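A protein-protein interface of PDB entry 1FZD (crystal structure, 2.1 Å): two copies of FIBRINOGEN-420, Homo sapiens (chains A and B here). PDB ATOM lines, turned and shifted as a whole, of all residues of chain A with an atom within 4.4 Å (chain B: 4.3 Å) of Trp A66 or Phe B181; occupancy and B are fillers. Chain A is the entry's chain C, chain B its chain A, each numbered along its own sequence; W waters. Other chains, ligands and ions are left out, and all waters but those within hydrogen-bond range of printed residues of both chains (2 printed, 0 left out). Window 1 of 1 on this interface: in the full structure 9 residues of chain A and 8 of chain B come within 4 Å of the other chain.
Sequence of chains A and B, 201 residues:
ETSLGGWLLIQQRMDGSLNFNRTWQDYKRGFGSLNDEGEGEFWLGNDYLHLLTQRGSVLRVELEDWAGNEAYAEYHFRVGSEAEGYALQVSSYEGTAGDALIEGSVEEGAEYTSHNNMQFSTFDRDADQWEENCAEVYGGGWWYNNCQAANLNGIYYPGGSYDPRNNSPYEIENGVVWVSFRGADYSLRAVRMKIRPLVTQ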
ATOM      1  N   ASP A  65       9.317  17.130 -19.740  1.00  0.00           N
ATOM      2  CA  ASP A  65       9.331  17.179 -18.274  1.00  0.00           C
ATOM      3  C   ASP A  65       8.069  17.919 -17.794  1.00  0.00           C
ATOM      4  O   ASP A  65       7.180  18.185 -18.619  1.00  0.00           O
ATOM      5  CB  ASP A  65      10.636  17.841 -17.864  1.00  0.00           C
ATOM      6  CG  ASP A  65      10.731  19.369 -17.971  1.00  0.00           C
ATOM      7  OD1 ASP A  65       9.834  20.101 -18.438  1.00  0.00           O
ATOM      8  OD2 ASP A  65      11.845  19.834 -17.591  1.00  0.00           O
ATOM      9  N   TRP A  66       7.886  18.033 -16.494  1.00  0.00           N
ATOM     10  CA  TRP A  66       6.670  18.602 -15.936  1.00  0.00           C
ATOM     11  C   TRP A  66       6.619  20.142 -16.007  1.00  0.00           C
ATOM     12  O   TRP A  66       5.587  20.664 -15.584  1.00  0.00           O
ATOM     13  CB  TRP A  66       6.511  18.141 -14.471  1.00  0.00           C
ATOM     14  CG  TRP A  66       6.190  16.678 -14.390  1.00  0.00           C
ATOM     15  CD1 TRP A  66       7.142  15.674 -14.466  1.00  0.00           C
ATOM     16  CD2 TRP A  66       4.924  16.033 -14.259  1.00  0.00           C
ATOM     17  NE1 TRP A  66       6.533  14.483 -14.334  1.00  0.00           N
ATOM     18  CE2 TRP A  66       5.175  14.648 -14.221  1.00  0.00           C
ATOM     19  CE3 TRP A  66       3.603  16.494 -14.149  1.00  0.00           C
ATOM     20  CZ2 TRP A  66       4.171  13.699 -14.111  1.00  0.00           C
ATOM     21  CZ3 TRP A  66       2.601  15.546 -14.034  1.00  0.00           C
ATOM     22  CH2 TRP A  66       2.875  14.141 -14.011  1.00  0.00           C
ATOM     23  N   ALA A  67       7.571  20.838 -16.600  1.00  0.00           N
ATOM     24  CA  ALA A  67       7.500  22.287 -16.770  1.00  0.00           C
ATOM     25  C   ALA A  67       7.494  22.675 -18.240  1.00  0.00           C
ATOM     26  O   ALA A  67       7.939  23.768 -18.562  1.00  0.00           O
ATOM     27  CB  ALA A  67       8.718  22.959 -16.161  1.00  0.00           C
ATOM     28  N   GLY A  68       7.068  21.789 -19.139  1.00  0.00           N
ATOM     29  CA  GLY A  68       7.091  22.096 -20.547  1.00  0.00           C
ATOM     30  C   GLY A  68       8.431  22.116 -21.255  1.00  0.00           C
ATOM     31  O   GLY A  68       8.344  22.414 -22.446  1.00  0.00           O
ATOM     32  N   TYR A 156       6.279   5.291 -12.979  1.00  0.00           N
ATOM     33  CA  TYR A 156       5.821   6.649 -13.202  1.00  0.00           C
ATOM     34  C   TYR A 156       5.607   7.413 -11.907  1.00  0.00           C
ATOM     35  O   TYR A 156       4.625   7.108 -11.245  1.00  0.00           O
ATOM     36  CB  TYR A 156       4.540   6.593 -14.067  1.00  0.00           C
ATOM     37  CG  TYR A 156       4.153   7.910 -14.697  1.00  0.00           C
ATOM     38  CD1 TYR A 156       3.396   8.868 -13.991  1.00  0.00           C
ATOM     39  CD2 TYR A 156       4.507   8.206 -16.014  1.00  0.00           C
ATOM     40  CE1 TYR A 156       3.041  10.077 -14.600  1.00  0.00           C
ATOM     41  CE2 TYR A 156       4.169   9.378 -16.615  1.00  0.00           C
ATOM     42  CZ  TYR A 156       3.383  10.319 -15.875  1.00  0.00           C
ATOM     43  OH  TYR A 156       3.043  11.481 -16.542  1.00  0.00           O
ATOM     44  N   TYR A 157       6.442   8.340 -11.477  1.00  0.00           N
ATOM     45  CA  TYR A 157       6.212   9.162 -10.271  1.00  0.00           C
ATOM     46  C   TYR A 157       5.631  10.525 -10.693  1.00  0.00           C
ATOM     47  O   TYR A 157       6.222  11.165 -11.559  1.00  0.00           O
ATOM     48  CB  TYR A 157       7.500   9.439  -9.494  1.00  0.00           C
ATOM     49  CG  TYR A 157       8.052   8.160  -8.864  1.00  0.00           C
ATOM     50  CD1 TYR A 157       7.431   7.504  -7.819  1.00  0.00           C
ATOM     51  CD2 TYR A 157       9.177   7.578  -9.453  1.00  0.00           C
ATOM     52  CE1 TYR A 157       7.970   6.327  -7.316  1.00  0.00           C
ATOM     53  CE2 TYR A 157       9.706   6.416  -8.980  1.00  0.00           C
ATOM     54  CZ  TYR A 157       9.131   5.802  -7.901  1.00  0.00           C
ATOM     55  OH  TYR A 157       9.687   4.644  -7.420  1.00  0.00           O
ATOM     56  N   PRO A 158       4.456  10.927 -10.252  1.00  0.00           N
ATOM     57  CA  PRO A 158       3.839  12.193 -10.588  1.00  0.00           C
ATOM     58  C   PRO A 158       4.550  13.436 -10.110  1.00  0.00           C
ATOM     59  O   PRO A 158       5.139  13.423  -9.039  1.00  0.00           O
ATOM     60  CB  PRO A 158       2.460  12.120  -9.927  1.00  0.00           C
ATOM     61  CG  PRO A 158       2.359  10.788  -9.285  1.00  0.00           C
ATOM     62  CD  PRO A 158       3.751  10.233  -9.126  1.00  0.00           C
ATOM     63  N   GLY A 159       4.542  14.539 -10.859  1.00  0.00           N
ATOM     64  CA  GLY A 159       5.132  15.783 -10.408  1.00  0.00           C
ATOM     65  C   GLY A 159       6.562  16.053 -10.859  1.00  0.00           C
ATOM     66  O   GLY A 159       6.939  17.239 -10.794  1.00  0.00           O
ATOM     67  N   GLY A 160       7.348  15.064 -11.300  1.00  0.00           N
ATOM     68  CA  GLY A 160       8.740  15.374 -11.682  1.00  0.00           C
ATOM     69  C   GLY A 160       9.702  14.839 -10.617  1.00  0.00           C
ATOM     70  O   GLY A 160       9.970  13.641 -10.477  1.00  0.00           O
ATOM     71  N   TYR A 186      14.629  12.557 -11.274  1.00  0.00           N
ATOM     72  CA  TYR A 186      13.489  13.328 -11.797  1.00  0.00           C
ATOM     73  C   TYR A 186      12.790  12.408 -12.805  1.00  0.00           C
ATOM     74  O   TYR A 186      13.443  11.960 -13.773  1.00  0.00           O
ATOM     75  CB  TYR A 186      13.945  14.629 -12.473  1.00  0.00           C
ATOM     76  CG  TYR A 186      12.849  15.525 -12.991  1.00  0.00           C
ATOM     77  CD1 TYR A 186      12.130  15.245 -14.129  1.00  0.00           C
ATOM     78  CD2 TYR A 186      12.594  16.764 -12.366  1.00  0.00           C
ATOM     79  CE1 TYR A 186      11.149  16.086 -14.583  1.00  0.00           C
ATOM     80  CE2 TYR A 186      11.617  17.643 -12.784  1.00  0.00           C
ATOM     81  CZ  TYR A 186      10.896  17.296 -13.908  1.00  0.00           C
ATOM     82  OH  TYR A 186       9.913  18.110 -14.422  1.00  0.00           O
ATOM     83  N   SER A 187      11.509  12.181 -12.583  1.00  0.00           N
ATOM     84  CA  SER A 187      10.703  11.333 -13.438  1.00  0.00           C
ATOM     85  C   SER A 187       9.948  12.118 -14.482  1.00  0.00           C
ATOM     86  O   SER A 187       9.172  13.011 -14.184  1.00  0.00           O
ATOM     87  CB  SER A 187       9.729  10.587 -12.511  1.00  0.00           C
ATOM     88  OG  SER A 187       9.214   9.446 -13.169  1.00  0.00           O
ATOM     89  N   LEU A 188       9.989  11.756 -15.733  1.00  0.00           N
ATOM     90  CA  LEU A 188       9.519  12.534 -16.858  1.00  0.00           C
ATOM     91  C   LEU A 188       8.010  12.395 -17.005  1.00  0.00           C
ATOM     92  O   LEU A 188       7.468  11.423 -16.496  1.00  0.00           O
ATOM     93  CB  LEU A 188      10.317  12.169 -18.108  1.00  0.00           C
ATOM     94  CG  LEU A 188      11.830  12.428 -18.087  1.00  0.00           C
ATOM     95  CD1 LEU A 188      12.550  11.717 -19.251  1.00  0.00           C
ATOM     96  CD2 LEU A 188      12.112  13.949 -18.192  1.00  0.00           C
ATOM     97  N   ARG A 189       7.371  13.326 -17.711  1.00  0.00           N
ATOM     98  CA  ARG A 189       5.916  13.366 -17.762  1.00  0.00           C
ATOM     99  C   ARG A 189       5.361  12.618 -18.967  1.00  0.00           C
ATOM    100  O   ARG A 189       4.390  11.943 -18.719  1.00  0.00           O
ATOM    101  CB  ARG A 189       5.377  14.814 -17.755  1.00  0.00           C
ATOM    102  CG  ARG A 189       3.908  15.025 -18.080  1.00  0.00           C
ATOM    103  CD  ARG A 189       3.388  16.452 -17.860  1.00  0.00           C
ATOM    104  NE  ARG A 189       3.870  17.467 -18.768  1.00  0.00           N
ATOM    105  CZ  ARG A 189       3.828  18.801 -18.764  1.00  0.00           C
ATOM    106  NH1 ARG A 189       3.313  19.483 -17.739  1.00  0.00           N
ATOM    107  NH2 ARG A 189       4.337  19.543 -19.761  1.00  0.00           N
ATOM    108  N   LEU B  63      -3.909  14.927  -1.110  1.00  0.00           N
ATOM    109  CA  LEU B  63      -4.359  14.523  -2.418  1.00  0.00           C
ATOM    110  C   LEU B  63      -4.102  13.020  -2.688  1.00  0.00           C
ATOM    111  O   LEU B  63      -3.012  12.568  -2.303  1.00  0.00           O
ATOM    112  CB  LEU B  63      -3.565  15.344  -3.498  1.00  0.00           C
ATOM    113  CG  LEU B  63      -3.510  16.887  -3.266  1.00  0.00           C
ATOM    114  CD1 LEU B  63      -2.421  17.535  -4.135  1.00  0.00           C
ATOM    115  CD2 LEU B  63      -4.833  17.555  -3.595  1.00  0.00           C
ATOM    116  N   ASN B  69      -0.758   6.940  -5.646  1.00  0.00           N
ATOM    117  CA  ASN B  69       0.184   7.943  -5.081  1.00  0.00           C
ATOM    118  C   ASN B  69      -0.588   9.007  -4.269  1.00  0.00           C
ATOM    119  O   ASN B  69      -1.688   9.458  -4.634  1.00  0.00           O
ATOM    120  CB  ASN B  69       0.901   8.686  -6.205  1.00  0.00           C
ATOM    121  CG  ASN B  69       1.545   7.677  -7.165  1.00  0.00           C
ATOM    122  OD1 ASN B  69       2.401   6.951  -6.687  1.00  0.00           O
ATOM    123  ND2 ASN B  69       1.151   7.534  -8.399  1.00  0.00           N
ATOM    124  N   GLU B  70       0.074   9.564  -3.261  1.00  0.00           N
ATOM    125  CA  GLU B  70      -0.416  10.576  -2.362  1.00  0.00           C
ATOM    126  C   GLU B  70       0.577  11.738  -2.188  1.00  0.00           C
ATOM    127  O   GLU B  70       1.768  11.557  -2.340  1.00  0.00           O
ATOM    128  CB  GLU B  70      -0.730  10.041  -0.963  1.00  0.00           C
ATOM    129  CG  GLU B  70      -1.636   8.832  -1.050  1.00  0.00           C
ATOM    130  CD  GLU B  70      -1.743   8.142   0.290  1.00  0.00           C
ATOM    131  OE1 GLU B  70      -2.492   8.674   1.130  1.00  0.00           O
ATOM    132  OE2 GLU B  70      -1.059   7.132   0.555  1.00  0.00           O
ATOM    133  N   ALA B  71       0.064  12.914  -1.945  1.00  0.00           N
ATOM    134  CA  ALA B  71       0.884  14.135  -1.746  1.00  0.00           C
ATOM    135  C   ALA B  71       0.124  15.068  -0.779  1.00  0.00           C
ATOM    136  O   ALA B  71      -1.096  14.866  -0.536  1.00  0.00           O
ATOM    137  CB  ALA B  71       1.131  14.790  -3.103  1.00  0.00           C
ATOM    138  N   ALA B  97       3.268  18.299  -2.552  1.00  0.00           N
ATOM    139  CA  ALA B  97       2.393  18.445  -3.720  1.00  0.00           C
ATOM    140  C   ALA B  97       2.795  19.550  -4.668  1.00  0.00           C
ATOM    141  O   ALA B  97       2.276  19.618  -5.780  1.00  0.00           O
ATOM    142  CB  ALA B  97       0.974  18.670  -3.234  1.00  0.00           C
ATOM    143  N   GLU B 107       4.192  26.840 -15.603  1.00  0.00           N
ATOM    144  CA  GLU B 107       4.039  27.054 -17.029  1.00  0.00           C
ATOM    145  C   GLU B 107       3.282  28.306 -17.371  1.00  0.00           C
ATOM    146  O   GLU B 107       3.683  28.913 -18.362  1.00  0.00           O
ATOM    147  CB  GLU B 107       3.352  25.857 -17.735  1.00  0.00           C
ATOM    148  CG  GLU B 107       4.219  24.606 -17.726  1.00  0.00           C
ATOM    149  CD  GLU B 107       3.784  23.571 -18.760  1.00  0.00           C
ATOM    150  OE1 GLU B 107       3.892  23.828 -19.983  1.00  0.00           O
ATOM    151  OE2 GLU B 107       3.342  22.501 -18.285  1.00  0.00           O
ATOM    152  N   TRP B 178      -4.779  19.679  -9.175  1.00  0.00           N
ATOM    153  CA  TRP B 178      -3.686  20.315  -8.462  1.00  0.00           C
ATOM    154  C   TRP B 178      -2.458  20.248  -9.406  1.00  0.00           C
ATOM    155  O   TRP B 178      -1.838  19.193  -9.630  1.00  0.00           O
ATOM    156  CB  TRP B 178      -3.407  19.696  -7.095  1.00  0.00           C
ATOM    157  CG  TRP B 178      -2.612  20.538  -6.120  1.00  0.00           C
ATOM    158  CD1 TRP B 178      -1.235  20.611  -6.136  1.00  0.00           C
ATOM    159  CD2 TRP B 178      -3.030  21.383  -5.043  1.00  0.00           C
ATOM    160  NE1 TRP B 178      -0.783  21.405  -5.121  1.00  0.00           N
ATOM    161  CE2 TRP B 178      -1.869  21.908  -4.446  1.00  0.00           C
ATOM    162  CE3 TRP B 178      -4.262  21.729  -4.504  1.00  0.00           C
ATOM    163  CZ2 TRP B 178      -1.860  22.779  -3.335  1.00  0.00           C
ATOM    164  CZ3 TRP B 178      -4.303  22.604  -3.403  1.00  0.00           C
ATOM    165  CH2 TRP B 178      -3.132  23.123  -2.825  1.00  0.00           C
ATOM    166  N   VAL B 179      -2.313  21.283 -10.233  1.00  0.00           N
ATOM    167  CA  VAL B 179      -1.465  21.269 -11.408  1.00  0.00           C
ATOM    168  C   VAL B 179      -0.055  20.810 -11.138  1.00  0.00           C
ATOM    169  O   VAL B 179       0.485  19.945 -11.834  1.00  0.00           O
ATOM    170  CB  VAL B 179      -1.493  22.600 -12.167  1.00  0.00           C
ATOM    171  CG1 VAL B 179      -0.596  23.612 -11.427  1.00  0.00           C
ATOM    172  CG2 VAL B 179      -1.027  22.451 -13.615  1.00  0.00           C
ATOM    173  N   SER B 180       0.580  21.213 -10.026  1.00  0.00           N
ATOM    174  CA  SER B 180       1.940  20.812  -9.791  1.00  0.00           C
ATOM    175  C   SER B 180       2.076  19.342  -9.400  1.00  0.00           C
ATOM    176  O   SER B 180       3.229  18.960  -9.298  1.00  0.00           O
ATOM    177  CB  SER B 180       2.630  21.683  -8.755  1.00  0.00           C
ATOM    178  OG  SER B 180       1.837  21.842  -7.627  1.00  0.00           O
ATOM    179  N   PHE B 181       1.027  18.619  -9.012  1.00  0.00           N
ATOM    180  CA  PHE B 181       1.161  17.222  -8.644  1.00  0.00           C
ATOM    181  C   PHE B 181       0.856  16.352  -9.886  1.00  0.00           C
ATOM    182  O   PHE B 181       1.706  15.526 -10.250  1.00  0.00           O
ATOM    183  CB  PHE B 181       0.206  16.840  -7.525  1.00  0.00           C
ATOM    184  CG  PHE B 181       0.092  15.420  -7.065  1.00  0.00           C
ATOM    185  CD1 PHE B 181       1.234  14.661  -6.794  1.00  0.00           C
ATOM    186  CD2 PHE B 181      -1.190  14.884  -6.828  1.00  0.00           C
ATOM    187  CE1 PHE B 181       1.154  13.340  -6.358  1.00  0.00           C
ATOM    188  CE2 PHE B 181      -1.267  13.581  -6.357  1.00  0.00           C
ATOM    189  CZ  PHE B 181      -0.127  12.820  -6.129  1.00  0.00           C
ATOM    190  N   ARG B 182      -0.304  16.546 -10.509  1.00  0.00           N
ATOM    191  CA  ARG B 182      -0.757  15.680 -11.545  1.00  0.00           C
ATOM    192  C   ARG B 182      -1.139  16.363 -12.850  1.00  0.00           C
ATOM    193  O   ARG B 182      -1.718  15.647 -13.678  1.00  0.00           O
ATOM    194  CB  ARG B 182      -1.952  14.790 -11.126  1.00  0.00           C
ATOM    195  CG  ARG B 182      -1.509  13.420 -10.597  1.00  0.00           C
ATOM    196  CD  ARG B 182      -1.078  12.495 -11.752  1.00  0.00           C
ATOM    197  NE  ARG B 182      -0.899  11.123 -11.258  1.00  0.00           N
ATOM    198  CZ  ARG B 182      -0.750  10.097 -12.130  1.00  0.00           C
ATOM    199  NH1 ARG B 182      -0.634  10.299 -13.423  1.00  0.00           N
ATOM    200  NH2 ARG B 182      -0.574   8.923 -11.563  1.00  0.00           N
ATOM    201  N   GLY B 183      -0.823  17.638 -13.002  1.00  0.00           N
ATOM    202  CA  GLY B 183      -1.182  18.345 -14.206  1.00  0.00           C
ATOM    203  C   GLY B 183      -2.625  18.837 -14.216  1.00  0.00           C
ATOM    204  O   GLY B 183      -3.418  18.387 -13.379  1.00  0.00           O
ATOM    205  N   LEU B 188      -8.338  14.041  -9.759  1.00  0.00           N
ATOM    206  CA  LEU B 188      -7.957  13.249  -8.612  1.00  0.00           C
ATOM    207  C   LEU B 188      -9.053  12.392  -7.962  1.00  0.00           C
ATOM    208  O   LEU B 188     -10.224  12.648  -8.173  1.00  0.00           O
ATOM    209  CB  LEU B 188      -7.295  14.121  -7.507  1.00  0.00           C
ATOM    210  CG  LEU B 188      -6.089  14.929  -8.059  1.00  0.00           C
ATOM    211  CD1 LEU B 188      -5.645  16.076  -7.155  1.00  0.00           C
ATOM    212  CD2 LEU B 188      -4.904  14.002  -8.368  1.00  0.00           C
HETATM  213  O   HOH W   1       5.397  19.402 -11.115  1.00  0.00           O
HETATM  214  O   HOH W   2       1.879   6.012 -10.660  1.00  0.00           O
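The backbone carbonyl oxygen (O) of Phe B181 sits at hydrogen-bond distance from the backbone NH (N) of Gly A159, 3.1 Å away.
The guanidinium group of Arg A189 is in salt-bridge range of the side-chain carboxylate of Glu B107, 3.1 Å away.
The side-chain hydroxyl (OH) of Tyr A156 lies within hydrogen-bond range of the backbone carbonyl oxygen (O) of Arg A189 (2.6 Å).
The side-chain hydroxyl (OH) of Tyr A186 lies within hydrogen-bond range of the backbone NH (N) of Trp A66 (2.9 Å).
OD1 of Asp A65 lies within hydrogen-bond range of N of Gly A68, 3.3 Å away.
The guanidinium group (NH2) of Arg A189 sits at hydrogen-bond distance from the backbone carbonyl oxygen (O) of Asp A65 (3.4 Å).
O of Ala B97 is in hydrogen-bond range of OG of Ser B180 (2.9 Å).
The side-chain carboxylate (OD1) of Asp A65 is in hydrogen-bond range of the backbone NH (N) of Ala A67.
Among the printed residues, merely in contact across the chains: Trp A66 with Glu B107 (3.96 Å), Trp A66 with Phe B181 (3.9 Å), Ala A67 with Glu B107 (3.8 Å), Gly A68 with Glu B107 (3.7 Å), Tyr A156 with Arg B182 (3.9 Å), Pro A158 with Asn B69 (3.6 Å), Pro A158 with Phe B181 (3.5 Å), Pro A158 with Arg B182 (3.7 Å) and Gly A159 with Ser B180 (3.9 Å).
Of the printed residues of chain B, Trp A66 touches Glu B107 (3.96 Å) and Phe B181 (3.9 Å).
Printed residues of chain A within 4 Å of Phe B181: Trp A66, Pro A158 and Gly A159.
Printed residues of chain B within 4 Å of Arg A189: Glu B107.
Of the printed residues of chain B, Gly A68 touches Glu B107 (3.7 Å).
Printed residues of chain B within 4 Å of Ala A67: Glu B107 (3.8 Å).
Printed residues of chain A within 4 Å of Arg B182: Tyr A156 (3.9 Å) and Pro A158 (3.7 Å).
Ala B97 touches none of the printed residues of chain A.
Gly A160 touches none of the printed residues of chain B.
The nearest printed residue of chain A that does not touch Phe B181 is Gly A160 (5.8 Å).
The nearest printed residue of chain B that does not touch Tyr A156 is Asn B69 (4.5 Å).
Of the 13 printed residues of chain B, 5 touch a printed residue of chain A.
Printed residues of chain B that touch a printed residue of chain A: Asn B69, Glu B107, Ser B180, Phe B181 and Arg B182.
Hydrophobic or aromatic side chains of chain B within 4 Å of the printed part of chain A: Phe B181.
Among the printed residues, 11 pairs touch across the chains.
Among the printed residues, Asp or Glu carboxylates within 4 Å of a Lys or Arg side-chain nitrogen of the other chain: Arg A189 with Glu B107.
Position printed for both chains: 188.
Water W1 bridges O of Gly A159 and O of Ser B180.
Water W2 lies within hydrogen-bond range of the side-chain amide nitrogen (ND2) of Asn B69 (2.8 Å) and the backbone carbonyl oxygen (O) of Tyr A156 (3.0 Å).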
